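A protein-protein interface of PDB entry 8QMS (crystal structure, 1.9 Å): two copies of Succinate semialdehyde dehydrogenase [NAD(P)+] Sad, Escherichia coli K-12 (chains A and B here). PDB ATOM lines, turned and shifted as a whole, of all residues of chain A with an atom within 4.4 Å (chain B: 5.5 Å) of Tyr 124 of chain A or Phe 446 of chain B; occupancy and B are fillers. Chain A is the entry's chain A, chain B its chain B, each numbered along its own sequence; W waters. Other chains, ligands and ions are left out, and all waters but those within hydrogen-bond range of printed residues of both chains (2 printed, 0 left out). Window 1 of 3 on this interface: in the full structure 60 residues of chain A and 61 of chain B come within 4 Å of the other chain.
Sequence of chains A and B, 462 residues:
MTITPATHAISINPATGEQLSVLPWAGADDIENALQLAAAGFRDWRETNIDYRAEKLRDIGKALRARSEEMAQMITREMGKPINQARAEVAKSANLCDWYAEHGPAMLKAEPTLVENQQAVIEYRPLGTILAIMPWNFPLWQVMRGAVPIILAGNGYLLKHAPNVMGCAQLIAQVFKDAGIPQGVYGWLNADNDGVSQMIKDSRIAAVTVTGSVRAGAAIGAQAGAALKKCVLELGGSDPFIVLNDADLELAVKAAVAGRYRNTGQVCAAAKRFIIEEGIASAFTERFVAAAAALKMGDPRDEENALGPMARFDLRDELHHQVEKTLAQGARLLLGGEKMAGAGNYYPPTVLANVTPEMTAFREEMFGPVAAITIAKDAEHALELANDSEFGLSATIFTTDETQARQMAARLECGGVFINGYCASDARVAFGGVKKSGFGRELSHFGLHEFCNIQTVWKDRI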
ATOM      1  N   LEU A 108     -29.641   4.949  -2.779  1.00  0.00           N
ATOM      2  CA  LEU A 108     -28.953   5.796  -1.816  1.00  0.00           C
ATOM      3  C   LEU A 108     -28.865   5.168  -0.433  1.00  0.00           C
ATOM      4  O   LEU A 108     -28.364   5.811   0.498  1.00  0.00           O
ATOM      5  CB  LEU A 108     -29.649   7.160  -1.730  1.00  0.00           C
ATOM      6  CG  LEU A 108     -29.519   8.014  -2.997  1.00  0.00           C
ATOM      7  CD1 LEU A 108     -30.400   9.254  -2.933  1.00  0.00           C
ATOM      8  CD2 LEU A 108     -28.070   8.406  -3.231  1.00  0.00           C
ATOM      9  N   LYS A 109     -29.326   3.933  -0.276  1.00  0.00           N
ATOM     10  CA  LYS A 109     -29.263   3.275   1.020  1.00  0.00           C
ATOM     11  C   LYS A 109     -27.823   2.973   1.410  1.00  0.00           C
ATOM     12  O   LYS A 109     -26.941   2.805   0.562  1.00  0.00           O
ATOM     13  CB  LYS A 109     -30.075   1.982   1.000  1.00  0.00           C
ATOM     14  CG  LYS A 109     -31.560   2.214   0.802  1.00  0.00           C
ATOM     15  CD  LYS A 109     -32.306   0.907   0.636  1.00  0.00           C
ATOM     16  CE  LYS A 109     -32.195   0.036   1.871  1.00  0.00           C
ATOM     17  NZ  LYS A 109     -33.028  -1.190   1.720  1.00  0.00           N
ATOM     18  N   GLU A 111     -24.529   1.081   2.458  1.00  0.00           N
ATOM     19  CA  GLU A 111     -23.963  -0.107   1.850  1.00  0.00           C
ATOM     20  C   GLU A 111     -23.230  -0.924   2.903  1.00  0.00           C
ATOM     21  O   GLU A 111     -22.342  -0.380   3.577  1.00  0.00           O
ATOM     22  CB  GLU A 111     -23.010   0.315   0.743  1.00  0.00           C
ATOM     23  CG  GLU A 111     -22.622  -0.725  -0.249  1.00  0.00           C
ATOM     24  CD  GLU A 111     -21.733  -0.138  -1.329  1.00  0.00           C
ATOM     25  OE1 GLU A 111     -22.262   0.515  -2.259  1.00  0.00           O
ATOM     26  OE2 GLU A 111     -20.499  -0.311  -1.235  1.00  0.00           O
ATOM     27  N   ILE A 122     -20.966   2.047   4.117  1.00  0.00           N
ATOM     28  CA  ILE A 122     -20.722   3.126   3.168  1.00  0.00           C
ATOM     29  C   ILE A 122     -22.002   3.941   3.050  1.00  0.00           C
ATOM     30  O   ILE A 122     -23.073   3.383   2.784  1.00  0.00           O
ATOM     31  CB  ILE A 122     -20.292   2.593   1.789  1.00  0.00           C
ATOM     32  CG1 ILE A 122     -19.132   1.592   1.905  1.00  0.00           C
ATOM     33  CG2 ILE A 122     -19.905   3.744   0.903  1.00  0.00           C
ATOM     34  CD1 ILE A 122     -17.852   2.174   2.503  1.00  0.00           C
ATOM     35  N   GLU A 123     -21.895   5.253   3.247  1.00  0.00           N
ATOM     36  CA  GLU A 123     -23.036   6.157   3.166  1.00  0.00           C
ATOM     37  C   GLU A 123     -22.889   7.075   1.961  1.00  0.00           C
ATOM     38  O   GLU A 123     -21.779   7.497   1.623  1.00  0.00           O
ATOM     39  CB  GLU A 123     -23.168   6.997   4.444  1.00  0.00           C
ATOM     40  CG  GLU A 123     -23.431   6.193   5.711  1.00  0.00           C
ATOM     41  CD  GLU A 123     -24.902   5.869   5.915  1.00  0.00           C
ATOM     42  OE1 GLU A 123     -25.715   6.122   4.993  1.00  0.00           O
ATOM     43  OE2 GLU A 123     -25.247   5.359   7.004  1.00  0.00           O
ATOM     44  N   TYR A 124     -24.014   7.389   1.319  1.00  0.00           N
ATOM     45  CA  TYR A 124     -24.041   8.251   0.133  1.00  0.00           C
ATOM     46  C   TYR A 124     -24.567   9.619   0.553  1.00  0.00           C
ATOM     47  O   TYR A 124     -25.775   9.860   0.579  1.00  0.00           O
ATOM     48  CB  TYR A 124     -24.888   7.622  -0.969  1.00  0.00           C
ATOM     49  CG  TYR A 124     -24.199   6.432  -1.587  1.00  0.00           C
ATOM     50  CD1 TYR A 124     -24.329   5.168  -1.031  1.00  0.00           C
ATOM     51  CD2 TYR A 124     -23.384   6.581  -2.699  1.00  0.00           C
ATOM     52  CE1 TYR A 124     -23.678   4.073  -1.583  1.00  0.00           C
ATOM     53  CE2 TYR A 124     -22.729   5.492  -3.261  1.00  0.00           C
ATOM     54  CZ  TYR A 124     -22.878   4.242  -2.695  1.00  0.00           C
ATOM     55  OH  TYR A 124     -22.232   3.158  -3.241  1.00  0.00           O
ATOM     56  N   ARG A 125     -23.626  10.539   0.890  1.00  0.00           N
ATOM     57  CA  ARG A 125     -24.004  11.851   1.393  1.00  0.00           C
ATOM     58  C   ARG A 125     -24.059  12.867   0.261  1.00  0.00           C
ATOM     59  O   ARG A 125     -23.367  12.718  -0.750  1.00  0.00           O
ATOM     60  CB  ARG A 125     -22.999  12.334   2.437  1.00  0.00           C
ATOM     61  CG  ARG A 125     -22.632  11.315   3.477  1.00  0.00           C
ATOM     62  CD  ARG A 125     -23.801  10.979   4.381  1.00  0.00           C
ATOM     63  NE  ARG A 125     -23.305  10.401   5.627  1.00  0.00           N
ATOM     64  CZ  ARG A 125     -24.060   9.807   6.539  1.00  0.00           C
ATOM     65  NH1 ARG A 125     -25.369   9.688   6.385  1.00  0.00           N
ATOM     66  NH2 ARG A 125     -23.484   9.321   7.638  1.00  0.00           N
ATOM     67  N   PRO A 126     -24.880  13.905   0.418  1.00  0.00           N
ATOM     68  CA  PRO A 126     -24.852  15.019  -0.536  1.00  0.00           C
ATOM     69  C   PRO A 126     -23.495  15.706  -0.522  1.00  0.00           C
ATOM     70  O   PRO A 126     -22.807  15.748   0.499  1.00  0.00           O
ATOM     71  CB  PRO A 126     -25.950  15.960  -0.021  1.00  0.00           C
ATOM     72  CG  PRO A 126     -26.800  15.126   0.876  1.00  0.00           C
ATOM     73  CD  PRO A 126     -25.893  14.095   1.469  1.00  0.00           C
ATOM     74  N   HIS A 449     -24.811   8.851  -8.079  1.00  0.00           N
ATOM     75  CA  HIS A 449     -23.654   8.733  -7.206  1.00  0.00           C
ATOM     76  C   HIS A 449     -22.501   9.647  -7.597  1.00  0.00           C
ATOM     77  O   HIS A 449     -21.639   9.913  -6.751  1.00  0.00           O
ATOM     78  CB  HIS A 449     -23.178   7.277  -7.180  1.00  0.00           C
ATOM     79  CG  HIS A 449     -24.128   6.346  -6.495  1.00  0.00           C
ATOM     80  ND1 HIS A 449     -24.069   4.977  -6.641  1.00  0.00           N
ATOM     81  CD2 HIS A 449     -25.155   6.589  -5.644  1.00  0.00           C
ATOM     82  CE1 HIS A 449     -25.019   4.416  -5.915  1.00  0.00           C
ATOM     83  NE2 HIS A 449     -25.691   5.372  -5.299  1.00  0.00           N
ATOM     84  N   CYS A 452     -22.246  12.449  -5.122  1.00  0.00           N
ATOM     85  CA  CYS A 452     -22.324  12.116  -3.709  1.00  0.00           C
ATOM     86  C   CYS A 452     -20.934  12.125  -3.098  1.00  0.00           C
ATOM     87  O   CYS A 452     -19.936  11.833  -3.766  1.00  0.00           O
ATOM     88  CB  CYS A 452     -22.948  10.738  -3.483  1.00  0.00           C
ATOM     89  SG  CYS A 452     -24.719  10.656  -3.750  1.00  0.00           S
ATOM     90  N   ASN A 453     -20.885  12.471  -1.814  1.00  0.00           N
ATOM     91  CA  ASN A 453     -19.735  12.196  -0.960  1.00  0.00           C
ATOM     92  C   ASN A 453     -19.903  10.769  -0.457  1.00  0.00           C
ATOM     93  O   ASN A 453     -20.738  10.493   0.405  1.00  0.00           O
ATOM     94  CB  ASN A 453     -19.663  13.212   0.179  1.00  0.00           C
ATOM     95  CG  ASN A 453     -18.801  12.740   1.361  1.00  0.00           C
ATOM     96  OD1 ASN A 453     -17.926  11.884   1.219  1.00  0.00           O
ATOM     97  ND2 ASN A 453     -19.057  13.312   2.535  1.00  0.00           N
ATOM     98  N   ILE A 454     -19.135   9.848  -1.025  1.00  0.00           N
ATOM     99  CA  ILE A 454     -19.158   8.462  -0.577  1.00  0.00           C
ATOM    100  C   ILE A 454     -18.348   8.388   0.713  1.00  0.00           C
ATOM    101  O   ILE A 454     -17.147   8.679   0.719  1.00  0.00           O
ATOM    102  CB  ILE A 454     -18.605   7.527  -1.663  1.00  0.00           C
ATOM    103  CG1 ILE A 454     -19.607   7.442  -2.826  1.00  0.00           C
ATOM    104  CG2 ILE A 454     -18.294   6.159  -1.086  1.00  0.00           C
ATOM    105  CD1 ILE A 454     -18.998   7.037  -4.148  1.00  0.00           C
ATOM    106  N   VAL B 429     -13.177  -0.791   2.644  1.00  0.00           N
ATOM    107  CA  VAL B 429     -13.973   0.428   2.744  1.00  0.00           C
ATOM    108  C   VAL B 429     -13.404   1.507   1.829  1.00  0.00           C
ATOM    109  O   VAL B 429     -12.227   1.487   1.457  1.00  0.00           O
ATOM    110  CB  VAL B 429     -14.069   0.957   4.198  1.00  0.00           C
ATOM    111  CG1 VAL B 429     -14.645  -0.113   5.125  1.00  0.00           C
ATOM    112  CG2 VAL B 429     -12.712   1.460   4.703  1.00  0.00           C
ATOM    113  N   ALA B 430     -14.271   2.456   1.465  1.00  0.00           N
ATOM    114  CA  ALA B 430     -13.881   3.563   0.605  1.00  0.00           C
ATOM    115  C   ALA B 430     -12.926   4.513   1.320  1.00  0.00           C
ATOM    116  O   ALA B 430     -13.003   4.724   2.538  1.00  0.00           O
ATOM    117  CB  ALA B 430     -15.115   4.338   0.135  1.00  0.00           C
ATOM    118  N   ARG B 441     -12.708   8.099  -5.176  1.00  0.00           N
ATOM    119  CA  ARG B 441     -12.638   7.164  -4.063  1.00  0.00           C
ATOM    120  C   ARG B 441     -11.730   5.996  -4.419  1.00  0.00           C
ATOM    121  O   ARG B 441     -11.731   5.522  -5.558  1.00  0.00           O
ATOM    122  CB  ARG B 441     -14.038   6.653  -3.685  1.00  0.00           C
ATOM    123  CG  ARG B 441     -14.945   7.723  -3.087  1.00  0.00           C
ATOM    124  CD  ARG B 441     -14.423   8.167  -1.722  1.00  0.00           C
ATOM    125  NE  ARG B 441     -15.230   9.227  -1.124  1.00  0.00           N
ATOM    126  CZ  ARG B 441     -14.985  10.523  -1.264  1.00  0.00           C
ATOM    127  NH1 ARG B 441     -14.004  10.963  -2.038  1.00  0.00           N
ATOM    128  NH2 ARG B 441     -15.740  11.401  -0.608  1.00  0.00           N
ATOM    129  N   GLU B 442     -10.951   5.541  -3.446  1.00  0.00           N
ATOM    130  CA  GLU B 442     -10.076   4.395  -3.635  1.00  0.00           C
ATOM    131  C   GLU B 442     -10.506   3.244  -2.732  1.00  0.00           C
ATOM    132  O   GLU B 442     -11.338   3.403  -1.834  1.00  0.00           O
ATOM    133  CB  GLU B 442      -8.613   4.784  -3.385  1.00  0.00           C
ATOM    134  CG  GLU B 442      -8.134   5.855  -4.359  1.00  0.00           C
ATOM    135  CD  GLU B 442      -6.629   5.929  -4.493  1.00  0.00           C
ATOM    136  OE1 GLU B 442      -5.955   4.882  -4.350  1.00  0.00           O
ATOM    137  OE2 GLU B 442      -6.120   7.043  -4.752  1.00  0.00           O
ATOM    138  N   LEU B 443      -9.943   2.066  -3.025  1.00  0.00           N
ATOM    139  CA  LEU B 443     -10.172   0.821  -2.293  1.00  0.00           C
ATOM    140  C   LEU B 443     -11.602   0.309  -2.454  1.00  0.00           C
ATOM    141  O   LEU B 443     -12.454   0.988  -3.037  1.00  0.00           O
ATOM    142  CB  LEU B 443      -9.804   0.990  -0.815  1.00  0.00           C
ATOM    143  CG  LEU B 443      -8.298   1.180  -0.610  1.00  0.00           C
ATOM    144  CD1 LEU B 443      -7.934   1.318   0.870  1.00  0.00           C
ATOM    145  CD2 LEU B 443      -7.510   0.033  -1.263  1.00  0.00           C
ATOM    146  N   SER B 444     -11.860  -0.898  -1.963  1.00  0.00           N
ATOM    147  CA  SER B 444     -13.121  -1.622  -2.172  1.00  0.00           C
ATOM    148  C   SER B 444     -13.420  -1.654  -3.676  1.00  0.00           C
ATOM    149  O   SER B 444     -12.504  -1.711  -4.505  1.00  0.00           O
ATOM    150  CB  SER B 444     -14.216  -1.016  -1.314  1.00  0.00           C
ATOM    151  OG  SER B 444     -15.366  -1.851  -1.301  1.00  0.00           O
ATOM    152  N   HIS B 445     -14.701  -1.619  -4.056  1.00  0.00           N
ATOM    153  CA  HIS B 445     -15.032  -1.608  -5.478  1.00  0.00           C
ATOM    154  C   HIS B 445     -14.856  -0.232  -6.102  1.00  0.00           C
ATOM    155  O   HIS B 445     -14.774  -0.130  -7.332  1.00  0.00           O
ATOM    156  CB  HIS B 445     -16.464  -2.117  -5.709  1.00  0.00           C
ATOM    157  CG  HIS B 445     -17.501  -1.453  -4.852  1.00  0.00           C
ATOM    158  ND1 HIS B 445     -18.077  -0.244  -5.179  1.00  0.00           N
ATOM    159  CD2 HIS B 445     -18.080  -1.841  -3.690  1.00  0.00           C
ATOM    160  CE1 HIS B 445     -18.960   0.086  -4.254  1.00  0.00           C
ATOM    161  NE2 HIS B 445     -18.983  -0.866  -3.339  1.00  0.00           N
ATOM    162  N   PHE B 446     -14.768   0.816  -5.277  1.00  0.00           N
ATOM    163  CA  PHE B 446     -14.601   2.171  -5.792  1.00  0.00           C
ATOM    164  C   PHE B 446     -13.273   2.319  -6.528  1.00  0.00           C
ATOM    165  O   PHE B 446     -13.227   2.841  -7.649  1.00  0.00           O
ATOM    166  CB  PHE B 446     -14.712   3.173  -4.636  1.00  0.00           C
ATOM    167  CG  PHE B 446     -15.928   2.959  -3.776  1.00  0.00           C
ATOM    168  CD1 PHE B 446     -17.155   3.486  -4.147  1.00  0.00           C
ATOM    169  CD2 PHE B 446     -15.849   2.206  -2.617  1.00  0.00           C
ATOM    170  CE1 PHE B 446     -18.281   3.278  -3.373  1.00  0.00           C
ATOM    171  CE2 PHE B 446     -16.972   1.990  -1.837  1.00  0.00           C
ATOM    172  CZ  PHE B 446     -18.190   2.531  -2.217  1.00  0.00           C
ATOM    173  N   GLY B 447     -12.179   1.850  -5.917  1.00  0.00           N
ATOM    174  CA  GLY B 447     -10.884   1.895  -6.582  1.00  0.00           C
ATOM    175  C   GLY B 447     -10.818   1.041  -7.836  1.00  0.00           C
ATOM    176  O   GLY B 447     -10.057   1.342  -8.759  1.00  0.00           O
ATOM    177  N   LEU B 448     -11.600  -0.041  -7.881  1.00  0.00           N
ATOM    178  CA  LEU B 448     -11.672  -0.864  -9.085  1.00  0.00           C
ATOM    179  C   LEU B 448     -12.381  -0.132 -10.219  1.00  0.00           C
ATOM    180  O   LEU B 448     -11.970  -0.231 -11.382  1.00  0.00           O
ATOM    181  CB  LEU B 448     -12.407  -2.171  -8.789  1.00  0.00           C
ATOM    182  CG  LEU B 448     -11.674  -3.445  -8.400  1.00  0.00           C
ATOM    183  CD1 LEU B 448     -12.676  -4.588  -8.375  1.00  0.00           C
ATOM    184  CD2 LEU B 448     -10.553  -3.729  -9.382  1.00  0.00           C
ATOM    185  N   HIS B 449     -13.454   0.598  -9.902  1.00  0.00           N
ATOM    186  CA  HIS B 449     -14.335   1.162 -10.920  1.00  0.00           C
ATOM    187  C   HIS B 449     -13.940   2.560 -11.378  1.00  0.00           C
ATOM    188  O   HIS B 449     -14.381   2.983 -12.455  1.00  0.00           O
ATOM    189  CB  HIS B 449     -15.776   1.208 -10.401  1.00  0.00           C
ATOM    190  CG  HIS B 449     -16.406  -0.141 -10.246  1.00  0.00           C
ATOM    191  ND1 HIS B 449     -17.576  -0.338  -9.543  1.00  0.00           N
ATOM    192  CD2 HIS B 449     -16.036  -1.356 -10.713  1.00  0.00           C
ATOM    193  CE1 HIS B 449     -17.894  -1.620  -9.577  1.00  0.00           C
ATOM    194  NE2 HIS B 449     -16.976  -2.259 -10.279  1.00  0.00           N
ATOM    195  N   GLU B 450     -13.143   3.292 -10.589  1.00  0.00           N
ATOM    196  CA  GLU B 450     -12.816   4.672 -10.943  1.00  0.00           C
ATOM    197  C   GLU B 450     -12.162   4.768 -12.313  1.00  0.00           C
ATOM    198  O   GLU B 450     -12.366   5.753 -13.031  1.00  0.00           O
ATOM    199  CB  GLU B 450     -11.897   5.302  -9.890  1.00  0.00           C
ATOM    200  CG  GLU B 450     -12.590   5.741  -8.604  1.00  0.00           C
ATOM    201  CD  GLU B 450     -13.386   7.032  -8.749  1.00  0.00           C
ATOM    202  OE1 GLU B 450     -13.505   7.551  -9.878  1.00  0.00           O
ATOM    203  OE2 GLU B 450     -13.901   7.533  -7.724  1.00  0.00           O
ATOM    204  N   PHE B 451     -11.375   3.770 -12.692  1.00  0.00           N
ATOM    205  CA  PHE B 451     -10.654   3.806 -13.956  1.00  0.00           C
ATOM    206  C   PHE B 451     -11.127   2.699 -14.883  1.00  0.00           C
ATOM    207  O   PHE B 451     -10.353   2.101 -15.634  1.00  0.00           O
ATOM    208  CB  PHE B 451      -9.150   3.768 -13.704  1.00  0.00           C
ATOM    209  CG  PHE B 451      -8.668   4.968 -12.947  1.00  0.00           C
ATOM    210  CD1 PHE B 451      -8.692   6.223 -13.546  1.00  0.00           C
ATOM    211  CD2 PHE B 451      -8.251   4.861 -11.626  1.00  0.00           C
ATOM    212  CE1 PHE B 451      -8.277   7.350 -12.851  1.00  0.00           C
ATOM    213  CE2 PHE B 451      -7.837   5.985 -10.922  1.00  0.00           C
ATOM    214  CZ  PHE B 451      -7.852   7.233 -11.534  1.00  0.00           C
HETATM  215  O   HOH W   1     -14.381   7.517   1.440  1.00  0.00           O
HETATM  216  O   HOH W   2     -17.433  10.631  -3.472  1.00  0.00           O
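NE of Arg 441 of chain B is in hydrogen-bond range of O of Ile 454 of chain A (2.7 Å). OE2 of Glu 111 of chain A sits at hydrogen-bond distance from NE2 of His 445 of chain B, 2.7 Å away. The guanidinium group (NH2) of Arg 441 of chain B is in hydrogen-bond range of the side-chain amide oxygen (OD1) of Asn 453 of chain A (2.9 Å).
The backbone carbonyl oxygen of Arg 125 of chain A is in hydrogen-bond range of the backbone NH of Asn 453 of chain A (2.7 Å). The side-chain carboxylate (OE1) of Glu 111 of chain A sits at hydrogen-bond distance from the side-chain hydroxyl (OH) of Tyr 124 of chain A (2.8 Å). N of Glu 111 of chain A sits at hydrogen-bond distance from O of Ile 122 of chain A. The backbone NH of Arg 441 of chain B sits at hydrogen-bond distance from the side-chain carboxylate of Glu 450 of chain B.
Glu 111 of chain A touches Phe 446 of chain B (OE2 to CZ, 3.8 Å). CD1 of Ile 122 of chain A touches N of Ala 430 of chain B (3.7 Å). Ile 122 of chain A touches Phe 446 of chain B. Phe 446 of chain B touches Tyr 124 of chain A. Ile 454 of chain A touches Ala 430 of chain B (CG2 to CB, 3.9 Å). Ile 454 of chain A touches Phe 446 of chain B.
Of the printed residues of chain B, Glu 111 of chain A touches His 445 and Phe 446. Of the printed residues of chain B, Ile 122 of chain A touches Ala 430 (3.7 Å) and Phe 446 (3.8 Å). Of chain B, only Phe 446 comes within 4 Å of Tyr 124 of chain A. Arg 125 of chain A touches none of the printed residues of chain B. Of the printed residues of chain B, Asn 453 of chain A touches Arg 441. Of the printed residues of chain A, His 445 of chain B touches Glu 111. Phe 446 of chain B touches four residues of chain A. Leu 448 of chain B touches none of the printed residues of chain A.
Of the 13 printed residues of chain B, 4 touch a printed residue of chain A. Hydrophobic or aromatic side chains of chain B that line the printed part of chain A: Ala 430, His 445 and Phe 446. Of the 12 printed residues of chain A, 5 touch a printed residue of chain B. Hydrophobic or aromatic side chains of chain A that line the printed part of chain B: Ile 122, Tyr 124 and Ile 454. Among the printed residues, 9 pairs touch across the chains. Among the printed residues, no Asp or Glu carboxylate lies within 4 Å of a Lys or Arg side-chain nitrogen of the other chain.
Position printed for both chains: 449. Of the 9 pairs that touch across the chains among the printed residues, none has its exchanged pair printed and touching as well.
Water W2 lies within hydrogen-bond range of O of Cys 452 of chain A (2.8 Å), N of Ile 454 of chain A (3.1 Å) and NH2 of Arg 441 of chain B (3.4 Å). Water W1 lies within hydrogen-bond range of the backbone carbonyl oxygen (O) of Ile 454 of chain A (3.1 Å), the guanidinium group (NE) of Arg 441 of chain B (3.2 Å) and the backbone carbonyl oxygen (O) of Ala 430 of chain B (3.3 Å).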
